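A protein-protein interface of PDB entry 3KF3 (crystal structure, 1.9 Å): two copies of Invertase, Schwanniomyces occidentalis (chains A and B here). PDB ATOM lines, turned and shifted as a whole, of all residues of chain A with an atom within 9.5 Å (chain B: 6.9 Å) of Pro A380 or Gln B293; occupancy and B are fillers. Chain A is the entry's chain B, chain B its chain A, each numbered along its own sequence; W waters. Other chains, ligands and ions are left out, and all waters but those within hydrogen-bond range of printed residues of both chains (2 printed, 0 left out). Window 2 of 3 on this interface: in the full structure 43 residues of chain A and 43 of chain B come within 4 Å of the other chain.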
ATOM      1  N   LEU A 376     -27.921 -29.623  17.409  1.00  0.00           N
ATOM      2  CA  LEU A 376     -28.526 -29.227  16.153  1.00  0.00           C
ATOM      3  C   LEU A 376     -27.420 -28.840  15.195  1.00  0.00           C
ATOM      4  O   LEU A 376     -26.539 -28.039  15.537  1.00  0.00           O
ATOM      5  CB  LEU A 376     -29.484 -28.046  16.342  1.00  0.00           C
ATOM      6  CG  LEU A 376     -30.196 -27.571  15.067  1.00  0.00           C
ATOM      7  CD1 LEU A 376     -31.252 -28.573  14.617  1.00  0.00           C
ATOM      8  CD2 LEU A 376     -30.807 -26.183  15.233  1.00  0.00           C
ATOM      9  N   ASN A 377     -27.471 -29.424  14.003  1.00  0.00           N
ATOM     10  CA  ASN A 377     -26.554 -29.092  12.932  1.00  0.00           C
ATOM     11  C   ASN A 377     -27.092 -27.917  12.142  1.00  0.00           C
ATOM     12  O   ASN A 377     -28.179 -27.975  11.567  1.00  0.00           O
ATOM     13  CB  ASN A 377     -26.323 -30.300  12.024  1.00  0.00           C
ATOM     14  CG  ASN A 377     -25.469 -31.367  12.682  1.00  0.00           C
ATOM     15  OD1 ASN A 377     -24.468 -31.066  13.339  1.00  0.00           O
ATOM     16  ND2 ASN A 377     -25.856 -32.627  12.504  1.00  0.00           N
ATOM     17  N   VAL A 378     -26.313 -26.846  12.132  1.00  0.00           N
ATOM     18  CA  VAL A 378     -26.715 -25.574  11.562  1.00  0.00           C
ATOM     19  C   VAL A 378     -25.589 -25.121  10.624  1.00  0.00           C
ATOM     20  O   VAL A 378     -24.450 -25.544  10.800  1.00  0.00           O
ATOM     21  CB  VAL A 378     -27.010 -24.585  12.725  1.00  0.00           C
ATOM     22  CG1 VAL A 378     -26.272 -23.272  12.588  1.00  0.00           C
ATOM     23  CG2 VAL A 378     -28.513 -24.389  12.905  1.00  0.00           C
ATOM     24  N   SER A 379     -25.898 -24.309   9.615  1.00  0.00           N
ATOM     25  CA  SER A 379     -24.865 -23.857   8.668  1.00  0.00           C
ATOM     26  C   SER A 379     -23.825 -22.976   9.377  1.00  0.00           C
ATOM     27  O   SER A 379     -24.172 -22.267  10.328  1.00  0.00           O
ATOM     28  CB  SER A 379     -25.488 -23.138   7.468  1.00  0.00           C
ATOM     29  OG  SER A 379     -26.111 -21.937   7.862  1.00  0.00           O
ATOM     30  N   PRO A 380     -22.554 -23.006   8.913  1.00  0.00           N
ATOM     31  CA  PRO A 380     -21.440 -22.476   9.726  1.00  0.00           C
ATOM     32  C   PRO A 380     -21.569 -21.000  10.110  1.00  0.00           C
ATOM     33  O   PRO A 380     -21.043 -20.583  11.142  1.00  0.00           O
ATOM     34  CB  PRO A 380     -20.205 -22.696   8.836  1.00  0.00           C
ATOM     35  CG  PRO A 380     -20.658 -23.613   7.724  1.00  0.00           C
ATOM     36  CD  PRO A 380     -22.113 -23.368   7.552  1.00  0.00           C
ATOM     37  N   GLY A 381     -22.269 -20.221   9.293  1.00  0.00           N
ATOM     38  CA  GLY A 381     -22.492 -18.815   9.596  1.00  0.00           C
ATOM     39  C   GLY A 381     -23.520 -18.539  10.681  1.00  0.00           C
ATOM     40  O   GLY A 381     -23.722 -17.385  11.059  1.00  0.00           O
ATOM     41  N   LYS A 382     -24.148 -19.593  11.201  1.00  0.00           N
ATOM     42  CA  LYS A 382     -25.266 -19.440  12.131  1.00  0.00           C
ATOM     43  C   LYS A 382     -25.060 -20.094  13.508  1.00  0.00           C
ATOM     44  O   LYS A 382     -25.983 -20.117  14.330  1.00  0.00           O
ATOM     45  CB  LYS A 382     -26.560 -19.954  11.478  1.00  0.00           C
ATOM     46  CG  LYS A 382     -27.049 -19.097  10.308  1.00  0.00           C
ATOM     47  CD  LYS A 382     -28.262 -19.696   9.615  1.00  0.00           C
ATOM     48  CE  LYS A 382     -28.626 -18.859   8.397  1.00  0.00           C
ATOM     49  NZ  LYS A 382     -29.516 -19.589   7.449  1.00  0.00           N
ATOM     50  N   THR A 383     -23.861 -20.608  13.766  1.00  0.00           N
ATOM     51  CA  THR A 383     -23.561 -21.276  15.037  1.00  0.00           C
ATOM     52  C   THR A 383     -23.308 -20.285  16.194  1.00  0.00           C
ATOM     53  O   THR A 383     -22.371 -20.460  16.981  1.00  0.00           O
ATOM     54  CB  THR A 383     -22.363 -22.253  14.903  1.00  0.00           C
ATOM     55  OG1 THR A 383     -21.204 -21.531  14.472  1.00  0.00           O
ATOM     56  CG2 THR A 383     -22.668 -23.353  13.896  1.00  0.00           C
ATOM     57  N   HIS A 384     -24.162 -19.270  16.309  1.00  0.00           N
ATOM     58  CA  HIS A 384     -23.989 -18.219  17.309  1.00  0.00           C
ATOM     59  C   HIS A 384     -25.295 -17.531  17.694  1.00  0.00           C
ATOM     60  O   HIS A 384     -26.291 -17.595  16.962  1.00  0.00           O
ATOM     61  CB  HIS A 384     -22.982 -17.169  16.811  1.00  0.00           C
ATOM     62  CG  HIS A 384     -23.473 -16.366  15.648  1.00  0.00           C
ATOM     63  ND1 HIS A 384     -23.394 -16.813  14.348  1.00  0.00           N
ATOM     64  CD2 HIS A 384     -24.050 -15.143  15.591  1.00  0.00           C
ATOM     65  CE1 HIS A 384     -23.896 -15.896  13.539  1.00  0.00           C
ATOM     66  NE2 HIS A 384     -24.302 -14.873  14.267  1.00  0.00           N
ATOM     67  N   PHE A 405     -21.797 -15.433  21.461  1.00  0.00           N
ATOM     68  CA  PHE A 405     -21.179 -16.727  21.717  1.00  0.00           C
ATOM     69  C   PHE A 405     -21.313 -17.579  20.461  1.00  0.00           C
ATOM     70  O   PHE A 405     -22.368 -17.594  19.827  1.00  0.00           O
ATOM     71  CB  PHE A 405     -21.843 -17.415  22.912  1.00  0.00           C
ATOM     72  CG  PHE A 405     -21.306 -18.791  23.203  1.00  0.00           C
ATOM     73  CD1 PHE A 405     -20.168 -18.956  23.976  1.00  0.00           C
ATOM     74  CD2 PHE A 405     -21.939 -19.924  22.695  1.00  0.00           C
ATOM     75  CE1 PHE A 405     -19.668 -20.222  24.241  1.00  0.00           C
ATOM     76  CE2 PHE A 405     -21.446 -21.189  22.957  1.00  0.00           C
ATOM     77  CZ  PHE A 405     -20.313 -21.340  23.736  1.00  0.00           C
ATOM     78  N   ASP A 406     -20.232 -18.250  20.084  1.00  0.00           N
ATOM     79  CA  ASP A 406     -20.252 -19.170  18.956  1.00  0.00           C
ATOM     80  C   ASP A 406     -20.040 -20.583  19.471  1.00  0.00           C
ATOM     81  O   ASP A 406     -19.008 -20.879  20.066  1.00  0.00           O
ATOM     82  CB  ASP A 406     -19.170 -18.806  17.932  1.00  0.00           C
ATOM     83  CG  ASP A 406     -19.295 -19.597  16.640  1.00  0.00           C
ATOM     84  OD1 ASP A 406     -19.110 -20.829  16.669  1.00  0.00           O
ATOM     85  OD2 ASP A 406     -19.571 -18.981  15.589  1.00  0.00           O
ATOM     86  N   SER A 407     -21.012 -21.455  19.225  1.00  0.00           N
ATOM     87  CA  SER A 407     -20.942 -22.836  19.713  1.00  0.00           C
ATOM     88  C   SER A 407     -19.875 -23.713  19.041  1.00  0.00           C
ATOM     89  O   SER A 407     -19.345 -24.626  19.683  1.00  0.00           O
ATOM     90  CB  SER A 407     -22.311 -23.505  19.603  1.00  0.00           C
ATOM     91  OG  SER A 407     -22.783 -23.412  18.274  1.00  0.00           O
ATOM     92  N   SER A 408     -19.558 -23.447  17.774  1.00  0.00           N
ATOM     93  CA  SER A 408     -18.483 -24.189  17.077  1.00  0.00           C
ATOM     94  C   SER A 408     -17.088 -23.894  17.659  1.00  0.00           C
ATOM     95  O   SER A 408     -16.210 -24.762  17.647  1.00  0.00           O
ATOM     96  CB  SER A 408     -18.495 -23.915  15.566  1.00  0.00           C
ATOM     97  OG  SER A 408     -18.028 -22.605  15.253  1.00  0.00           O
ATOM     98  N   GLN A 409     -16.909 -22.677  18.172  1.00  0.00           N
ATOM     99  CA  GLN A 409     -15.636 -22.223  18.748  1.00  0.00           C
ATOM    100  C   GLN A 409     -15.598 -22.249  20.279  1.00  0.00           C
ATOM    101  O   GLN A 409     -14.545 -22.007  20.874  1.00  0.00           O
ATOM    102  CB  GLN A 409     -15.322 -20.797  18.270  1.00  0.00           C
ATOM    103  CG  GLN A 409     -15.296 -20.636  16.760  1.00  0.00           C
ATOM    104  CD  GLN A 409     -14.437 -21.678  16.078  1.00  0.00           C
ATOM    105  OE1 GLN A 409     -14.934 -22.477  15.280  1.00  0.00           O
ATOM    106  NE2 GLN A 409     -13.146 -21.691  16.401  1.00  0.00           N
ATOM    107  N   TYR A 413     -17.524 -13.554  22.354  1.00  0.00           N
ATOM    108  CA  TYR A 413     -16.875 -12.443  21.659  1.00  0.00           C
ATOM    109  C   TYR A 413     -17.585 -11.123  21.941  1.00  0.00           C
ATOM    110  O   TYR A 413     -18.780 -11.088  22.280  1.00  0.00           O
ATOM    111  CB  TYR A 413     -16.797 -12.703  20.138  1.00  0.00           C
ATOM    112  CG  TYR A 413     -18.129 -13.055  19.516  1.00  0.00           C
ATOM    113  CD1 TYR A 413     -19.007 -12.061  19.082  1.00  0.00           C
ATOM    114  CD2 TYR A 413     -18.518 -14.389  19.372  1.00  0.00           C
ATOM    115  CE1 TYR A 413     -20.242 -12.391  18.523  1.00  0.00           C
ATOM    116  CE2 TYR A 413     -19.737 -14.721  18.817  1.00  0.00           C
ATOM    117  CZ  TYR A 413     -20.595 -13.726  18.389  1.00  0.00           C
ATOM    118  OH  TYR A 413     -21.816 -14.071  17.840  1.00  0.00           O
ATOM    119  N   ASP A 491     -29.732 -16.325  14.219  1.00  0.00           N
ATOM    120  CA  ASP A 491     -30.207 -16.525  12.851  1.00  0.00           C
ATOM    121  C   ASP A 491     -30.707 -17.943  12.596  1.00  0.00           C
ATOM    122  O   ASP A 491     -31.235 -18.222  11.526  1.00  0.00           O
ATOM    123  CB  ASP A 491     -29.120 -16.180  11.830  1.00  0.00           C
ATOM    124  CG  ASP A 491     -28.824 -14.702  11.771  1.00  0.00           C
ATOM    125  OD1 ASP A 491     -29.756 -13.883  11.934  1.00  0.00           O
ATOM    126  OD2 ASP A 491     -27.646 -14.364  11.548  1.00  0.00           O
ATOM    127  N   THR A 492     -30.544 -18.830  13.570  1.00  0.00           N
ATOM    128  CA  THR A 492     -30.983 -20.208  13.411  1.00  0.00           C
ATOM    129  C   THR A 492     -32.510 -20.272  13.351  1.00  0.00           C
ATOM    130  O   THR A 492     -33.197 -19.568  14.099  1.00  0.00           O
ATOM    131  CB  THR A 492     -30.456 -21.123  14.540  1.00  0.00           C
ATOM    132  OG1 THR A 492     -31.083 -20.777  15.784  1.00  0.00           O
ATOM    133  CG2 THR A 492     -28.944 -20.991  14.681  1.00  0.00           C
ATOM    134  N   LEU A 496     -30.715 -23.798  18.418  1.00  0.00           N
ATOM    135  CA  LEU A 496     -29.373 -24.282  18.759  1.00  0.00           C
ATOM    136  C   LEU A 496     -29.030 -23.945  20.213  1.00  0.00           C
ATOM    137  O   LEU A 496     -28.242 -24.648  20.855  1.00  0.00           O
ATOM    138  CB  LEU A 496     -28.331 -23.683  17.800  1.00  0.00           C
ATOM    139  CG  LEU A 496     -26.825 -23.862  18.025  1.00  0.00           C
ATOM    140  CD1 LEU A 496     -26.399 -25.328  18.117  1.00  0.00           C
ATOM    141  CD2 LEU A 496     -26.076 -23.151  16.902  1.00  0.00           C
ATOM    142  N   TRP B  21      -8.245 -28.914   1.004  1.00  0.00           N
ATOM    143  CA  TRP B  21      -7.929 -28.274   2.277  1.00  0.00           C
ATOM    144  C   TRP B  21      -6.510 -28.586   2.741  1.00  0.00           C
ATOM    145  O   TRP B  21      -6.070 -29.734   2.669  1.00  0.00           O
ATOM    146  CB  TRP B  21      -8.932 -28.728   3.344  1.00  0.00           C
ATOM    147  CG  TRP B  21      -8.452 -28.503   4.747  1.00  0.00           C
ATOM    148  CD1 TRP B  21      -7.729 -29.370   5.513  1.00  0.00           C
ATOM    149  CD2 TRP B  21      -8.647 -27.327   5.545  1.00  0.00           C
ATOM    150  NE1 TRP B  21      -7.461 -28.808   6.739  1.00  0.00           N
ATOM    151  CE2 TRP B  21      -8.013 -27.555   6.785  1.00  0.00           C
ATOM    152  CE3 TRP B  21      -9.287 -26.101   5.328  1.00  0.00           C
ATOM    153  CZ2 TRP B  21      -8.010 -26.608   7.813  1.00  0.00           C
ATOM    154  CZ3 TRP B  21      -9.278 -25.156   6.345  1.00  0.00           C
ATOM    155  CH2 TRP B  21      -8.647 -25.418   7.577  1.00  0.00           C
ATOM    156  N   THR B  48     -12.989 -28.405   0.935  1.00  0.00           N
ATOM    157  CA  THR B  48     -12.269 -27.196   1.314  1.00  0.00           C
ATOM    158  C   THR B  48     -12.399 -26.960   2.835  1.00  0.00           C
ATOM    159  O   THR B  48     -12.508 -25.824   3.305  1.00  0.00           O
ATOM    160  CB  THR B  48     -12.729 -25.989   0.458  1.00  0.00           C
ATOM    161  OG1 THR B  48     -12.265 -24.770   1.040  1.00  0.00           O
ATOM    162  CG2 THR B  48     -14.229 -25.932   0.364  1.00  0.00           C
ATOM    163  N   ALA B  49     -12.388 -28.064   3.584  1.00  0.00           N
ATOM    164  CA  ALA B  49     -12.419 -28.053   5.038  1.00  0.00           C
ATOM    165  C   ALA B  49     -11.762 -29.319   5.577  1.00  0.00           C
ATOM    166  O   ALA B  49     -11.620 -30.313   4.855  1.00  0.00           O
ATOM    167  CB  ALA B  49     -13.856 -27.933   5.550  1.00  0.00           C
ATOM    168  N   GLN B 289      -9.866 -20.412  14.093  1.00  0.00           N
ATOM    169  CA  GLN B 289     -11.160 -19.750  14.320  1.00  0.00           C
ATOM    170  C   GLN B 289     -11.978 -19.602  13.048  1.00  0.00           C
ATOM    171  O   GLN B 289     -13.205 -19.703  13.079  1.00  0.00           O
ATOM    172  CB  GLN B 289     -10.971 -18.358  14.922  1.00  0.00           C
ATOM    173  CG  GLN B 289     -10.594 -18.343  16.387  1.00  0.00           C
ATOM    174  CD  GLN B 289     -10.330 -16.936  16.871  1.00  0.00           C
ATOM    175  OE1 GLN B 289      -9.791 -16.112  16.133  1.00  0.00           O
ATOM    176  NE2 GLN B 289     -10.727 -16.643  18.109  1.00  0.00           N
ATOM    177  N   TYR B 290     -11.303 -19.361  11.928  1.00  0.00           N
ATOM    178  CA  TYR B 290     -12.004 -19.050  10.680  1.00  0.00           C
ATOM    179  C   TYR B 290     -11.388 -19.643   9.416  1.00  0.00           C
ATOM    180  O   TYR B 290     -11.907 -19.422   8.324  1.00  0.00           O
ATOM    181  CB  TYR B 290     -12.116 -17.535  10.514  1.00  0.00           C
ATOM    182  CG  TYR B 290     -10.822 -16.797  10.758  1.00  0.00           C
ATOM    183  CD1 TYR B 290      -9.767 -16.870   9.841  1.00  0.00           C
ATOM    184  CD2 TYR B 290     -10.650 -16.013  11.903  1.00  0.00           C
ATOM    185  CE1 TYR B 290      -8.570 -16.195  10.063  1.00  0.00           C
ATOM    186  CE2 TYR B 290      -9.454 -15.323  12.134  1.00  0.00           C
ATOM    187  CZ  TYR B 290      -8.419 -15.419  11.206  1.00  0.00           C
ATOM    188  OH  TYR B 290      -7.238 -14.730  11.411  1.00  0.00           O
ATOM    189  N   ALA B 291     -10.300 -20.392   9.571  1.00  0.00           N
ATOM    190  CA  ALA B 291      -9.571 -21.003   8.451  1.00  0.00           C
ATOM    191  C   ALA B 291     -10.452 -21.702   7.396  1.00  0.00           C
ATOM    192  O   ALA B 291     -10.202 -21.562   6.192  1.00  0.00           O
ATOM    193  CB  ALA B 291      -8.504 -21.983   8.993  1.00  0.00           C
ATOM    194  N   ASP B 292     -11.462 -22.450   7.840  1.00  0.00           N
ATOM    195  CA  ASP B 292     -12.306 -23.203   6.904  1.00  0.00           C
ATOM    196  C   ASP B 292     -13.507 -22.425   6.342  1.00  0.00           C
ATOM    197  O   ASP B 292     -14.383 -23.008   5.707  1.00  0.00           O
ATOM    198  CB  ASP B 292     -12.724 -24.571   7.484  1.00  0.00           C
ATOM    199  CG  ASP B 292     -13.694 -24.470   8.668  1.00  0.00           C
ATOM    200  OD1 ASP B 292     -14.106 -25.547   9.147  1.00  0.00           O
ATOM    201  OD2 ASP B 292     -14.052 -23.359   9.126  1.00  0.00           O
ATOM    202  N   GLN B 293     -13.520 -21.112   6.560  1.00  0.00           N
ATOM    203  CA  GLN B 293     -14.647 -20.267   6.164  1.00  0.00           C
ATOM    204  C   GLN B 293     -14.273 -19.123   5.229  1.00  0.00           C
ATOM    205  O   GLN B 293     -15.151 -18.471   4.682  1.00  0.00           O
ATOM    206  CB  GLN B 293     -15.348 -19.698   7.407  1.00  0.00           C
ATOM    207  CG  GLN B 293     -15.895 -20.755   8.353  1.00  0.00           C
ATOM    208  CD  GLN B 293     -16.874 -21.671   7.670  1.00  0.00           C
ATOM    209  OE1 GLN B 293     -17.669 -21.233   6.842  1.00  0.00           O
ATOM    210  NE2 GLN B 293     -16.815 -22.954   8.001  1.00  0.00           N
ATOM    211  N   VAL B 294     -12.977 -18.885   5.047  1.00  0.00           N
ATOM    212  CA  VAL B 294     -12.507 -17.768   4.222  1.00  0.00           C
ATOM    213  C   VAL B 294     -12.886 -17.957   2.737  1.00  0.00           C
ATOM    214  O   VAL B 294     -12.959 -19.093   2.264  1.00  0.00           O
ATOM    215  CB  VAL B 294     -10.974 -17.521   4.408  1.00  0.00           C
ATOM    216  CG1 VAL B 294     -10.640 -17.292   5.879  1.00  0.00           C
ATOM    217  CG2 VAL B 294     -10.137 -18.681   3.829  1.00  0.00           C
ATOM    218  N   PRO B 295     -13.135 -16.849   2.002  1.00  0.00           N
ATOM    219  CA  PRO B 295     -13.689 -16.970   0.647  1.00  0.00           C
ATOM    220  C   PRO B 295     -12.660 -17.272  -0.462  1.00  0.00           C
ATOM    221  O   PRO B 295     -12.448 -16.449  -1.373  1.00  0.00           O
ATOM    222  CB  PRO B 295     -14.340 -15.604   0.427  1.00  0.00           C
ATOM    223  CG  PRO B 295     -13.483 -14.674   1.186  1.00  0.00           C
ATOM    224  CD  PRO B 295     -13.048 -15.438   2.423  1.00  0.00           C
ATOM    225  N   THR B 296     -12.029 -18.440  -0.367  1.00  0.00           N
ATOM    226  CA  THR B 296     -11.229 -18.987  -1.457  1.00  0.00           C
ATOM    227  C   THR B 296     -11.801 -20.325  -1.897  1.00  0.00           C
ATOM    228  O   THR B 296     -12.395 -21.055  -1.093  1.00  0.00           O
ATOM    229  CB  THR B 296      -9.754 -19.190  -1.063  1.00  0.00           C
ATOM    230  OG1 THR B 296      -9.669 -20.076   0.061  1.00  0.00           O
ATOM    231  CG2 THR B 296      -9.112 -17.858  -0.720  1.00  0.00           C
ATOM    232  N   ARG B 300      -8.420 -24.112   0.247  1.00  0.00           N
ATOM    233  CA  ARG B 300      -8.254 -23.192   1.370  1.00  0.00           C
ATOM    234  C   ARG B 300      -6.891 -23.378   2.018  1.00  0.00           C
ATOM    235  O   ARG B 300      -6.445 -24.513   2.219  1.00  0.00           O
ATOM    236  CB  ARG B 300      -9.356 -23.362   2.425  1.00  0.00           C
ATOM    237  CG  ARG B 300     -10.612 -22.551   2.146  1.00  0.00           C
ATOM    238  CD  ARG B 300     -11.598 -22.592   3.315  1.00  0.00           C
ATOM    239  NE  ARG B 300     -12.782 -21.782   3.019  1.00  0.00           N
ATOM    240  CZ  ARG B 300     -13.976 -22.260   2.670  1.00  0.00           C
ATOM    241  NH1 ARG B 300     -14.195 -23.565   2.584  1.00  0.00           N
ATOM    242  NH2 ARG B 300     -14.972 -21.421   2.415  1.00  0.00           N
ATOM    243  N   GLU B 422     -18.157 -10.585   3.588  1.00  0.00           N
ATOM    244  CA  GLU B 422     -18.701 -11.351   4.704  1.00  0.00           C
ATOM    245  C   GLU B 422     -18.395 -12.817   4.552  1.00  0.00           C
ATOM    246  O   GLU B 422     -18.429 -13.342   3.450  1.00  0.00           O
ATOM    247  CB  GLU B 422     -20.220 -11.182   4.786  1.00  0.00           C
ATOM    248  CG  GLU B 422     -20.683 -10.251   5.881  1.00  0.00           C
ATOM    249  CD  GLU B 422     -19.994  -8.904   5.830  1.00  0.00           C
ATOM    250  OE1 GLU B 422     -19.385  -8.509   6.854  1.00  0.00           O
ATOM    251  OE2 GLU B 422     -20.053  -8.249   4.761  1.00  0.00           O
ATOM    252  N   PHE B 423     -18.104 -13.471   5.667  1.00  0.00           N
ATOM    253  CA  PHE B 423     -17.982 -14.930   5.707  1.00  0.00           C
ATOM    254  C   PHE B 423     -18.197 -15.431   7.131  1.00  0.00           C
ATOM    255  O   PHE B 423     -18.020 -14.668   8.081  1.00  0.00           O
ATOM    256  CB  PHE B 423     -16.647 -15.421   5.115  1.00  0.00           C
ATOM    257  CG  PHE B 423     -15.426 -14.731   5.673  1.00  0.00           C
ATOM    258  CD1 PHE B 423     -14.863 -13.643   5.009  1.00  0.00           C
ATOM    259  CD2 PHE B 423     -14.825 -15.186   6.840  1.00  0.00           C
ATOM    260  CE1 PHE B 423     -13.713 -13.007   5.513  1.00  0.00           C
ATOM    261  CE2 PHE B 423     -13.691 -14.551   7.361  1.00  0.00           C
ATOM    262  CZ  PHE B 423     -13.131 -13.465   6.691  1.00  0.00           C
ATOM    263  N   PRO B 424     -18.592 -16.707   7.289  1.00  0.00           N
ATOM    264  CA  PRO B 424     -18.852 -17.218   8.633  1.00  0.00           C
ATOM    265  C   PRO B 424     -17.674 -17.054   9.594  1.00  0.00           C
ATOM    266  O   PRO B 424     -16.513 -17.167   9.193  1.00  0.00           O
ATOM    267  CB  PRO B 424     -19.142 -18.701   8.386  1.00  0.00           C
ATOM    268  CG  PRO B 424     -19.744 -18.726   7.016  1.00  0.00           C
ATOM    269  CD  PRO B 424     -18.963 -17.689   6.251  1.00  0.00           C
ATOM    270  N   ARG B 425     -18.001 -16.770  10.855  1.00  0.00           N
ATOM    271  CA  ARG B 425     -17.037 -16.645  11.963  1.00  0.00           C
ATOM    272  C   ARG B 425     -16.109 -15.440  11.868  1.00  0.00           C
ATOM    273  O   ARG B 425     -15.038 -15.412  12.482  1.00  0.00           O
ATOM    274  CB  ARG B 425     -16.247 -17.940  12.175  1.00  0.00           C
ATOM    275  CG  ARG B 425     -17.149 -19.119  12.413  1.00  0.00           C
ATOM    276  CD  ARG B 425     -16.458 -20.217  13.157  1.00  0.00           C
ATOM    277  NE  ARG B 425     -16.901 -21.490  12.608  1.00  0.00           N
ATOM    278  CZ  ARG B 425     -16.137 -22.319  11.909  1.00  0.00           C
ATOM    279  NH1 ARG B 425     -14.846 -22.053  11.693  1.00  0.00           N
ATOM    280  NH2 ARG B 425     -16.676 -23.435  11.449  1.00  0.00           N
ATOM    281  N   LYS B 426     -16.543 -14.429  11.128  1.00  0.00           N
ATOM    282  CA  LYS B 426     -15.779 -13.207  11.008  1.00  0.00           C
ATOM    283  C   LYS B 426     -15.774 -12.397  12.313  1.00  0.00           C
ATOM    284  O   LYS B 426     -15.010 -11.444  12.458  1.00  0.00           O
ATOM    285  CB  LYS B 426     -16.261 -12.374   9.825  1.00  0.00           C
ATOM    286  CG  LYS B 426     -15.141 -11.529   9.226  1.00  0.00           C
ATOM    287  CD  LYS B 426     -15.579 -10.689   8.045  1.00  0.00           C
ATOM    288  CE  LYS B 426     -14.499  -9.653   7.733  1.00  0.00           C
ATOM    289  NZ  LYS B 426     -14.790  -8.834   6.520  1.00  0.00           N
HETATM  290  O   HOH W   1     -20.502 -16.498  11.992  1.00  0.00           O
HETATM  291  O   HOH W   2     -19.487 -22.437  12.521  1.00  0.00           O
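NE of Arg B425 lies close to OE1 of Gln A409 (3.5 Å). NE of Arg B425 is in hydrogen-bond range of OG of Ser A408 (3.1 Å).
ND1 of His A384 lies close to O of Gly A381 (3.4 Å). The side-chain carboxylate (OD2) of Asp B292 is in hydrogen-bond range of the side-chain amide nitrogen (NE2) of Gln B293 (3.0 Å). The side-chain carboxylate (OD1) of Asp A406 sits at hydrogen-bond distance from the backbone NH (N) of Gln A409 (3.2 Å). The side-chain hydroxyl (OG1) of Thr A383 sits at hydrogen-bond distance from the backbone carbonyl oxygen (O) of Pro A380 (3.5 Å). NE2 of Gln B293 lies close to NH2 of Arg B425 (3.5 Å). The side-chain carboxylate (OD1) of Asp A406 is in hydrogen-bond range of the side-chain hydroxyl (OG) of Ser A408, 2.5 Å away.
Pro A380 touches Gln B293. Pro B424 touches Pro A380. Pro B424 touches Gly A381. OD2 of Asp A406 touches CG of Arg B425 (3.997 Å). CA of Gln B289 touches NE2 of Gln A409, 3.5 Å away.
Printed residues of chain B within 4 Å of Pro A380: Gln B293 (3.5 Å) and Pro B424 (3.8 Å). Of the printed residues of chain B, Asp A406 touches Arg B425. Asp A491 touches none of the printed residues of chain B. Tyr B290 touches none of the printed residues of chain A. Gln B293 touches one residue of chain A. No residue of chain A comes within 4 Å of Val B294. Pro B424 touches just these residues of chain A: Pro A380 (3.8 Å) and Gly A381 (3.6 Å). Printed residues of chain A within 4 Å of Arg B425: Asp A406, Ser A408 and Gln A409. The nearest residue of chain B that does not touch Pro A380 is Arg B425 (4.3 Å). The nearest residue of chain A that does not touch Gln B293 is Gly A381 (5.3 Å).
Printed residues of chain B that touch a printed residue of chain A: Gln B289, Gln B293, Pro B424 and Arg B425. Of the 18 printed residues of chain A, 5 touch a printed residue of chain B. Printed residues of chain A that touch a printed residue of chain B: Pro A380, Gly A381, Asp A406, Ser A408 and Gln A409.
No position is printed for both chains. Of the 7 pairs that touch across the chains among the printed residues, none has its exchanged pair printed and touching as well.
Water W2 lies within hydrogen-bond range of the side-chain hydroxyl (OG1) of Thr A383 (2.8 Å), the guanidinium group (NE) of Arg B425 (2.8 Å), the backbone carbonyl oxygen (O) of Pro A380 (2.8 Å) and the side-chain hydroxyl (OG) of Ser A408 (3.1 Å). Water W1 bridges N of Arg B425 (2.8 Å) and O of Gly A381 (3.5 Å).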
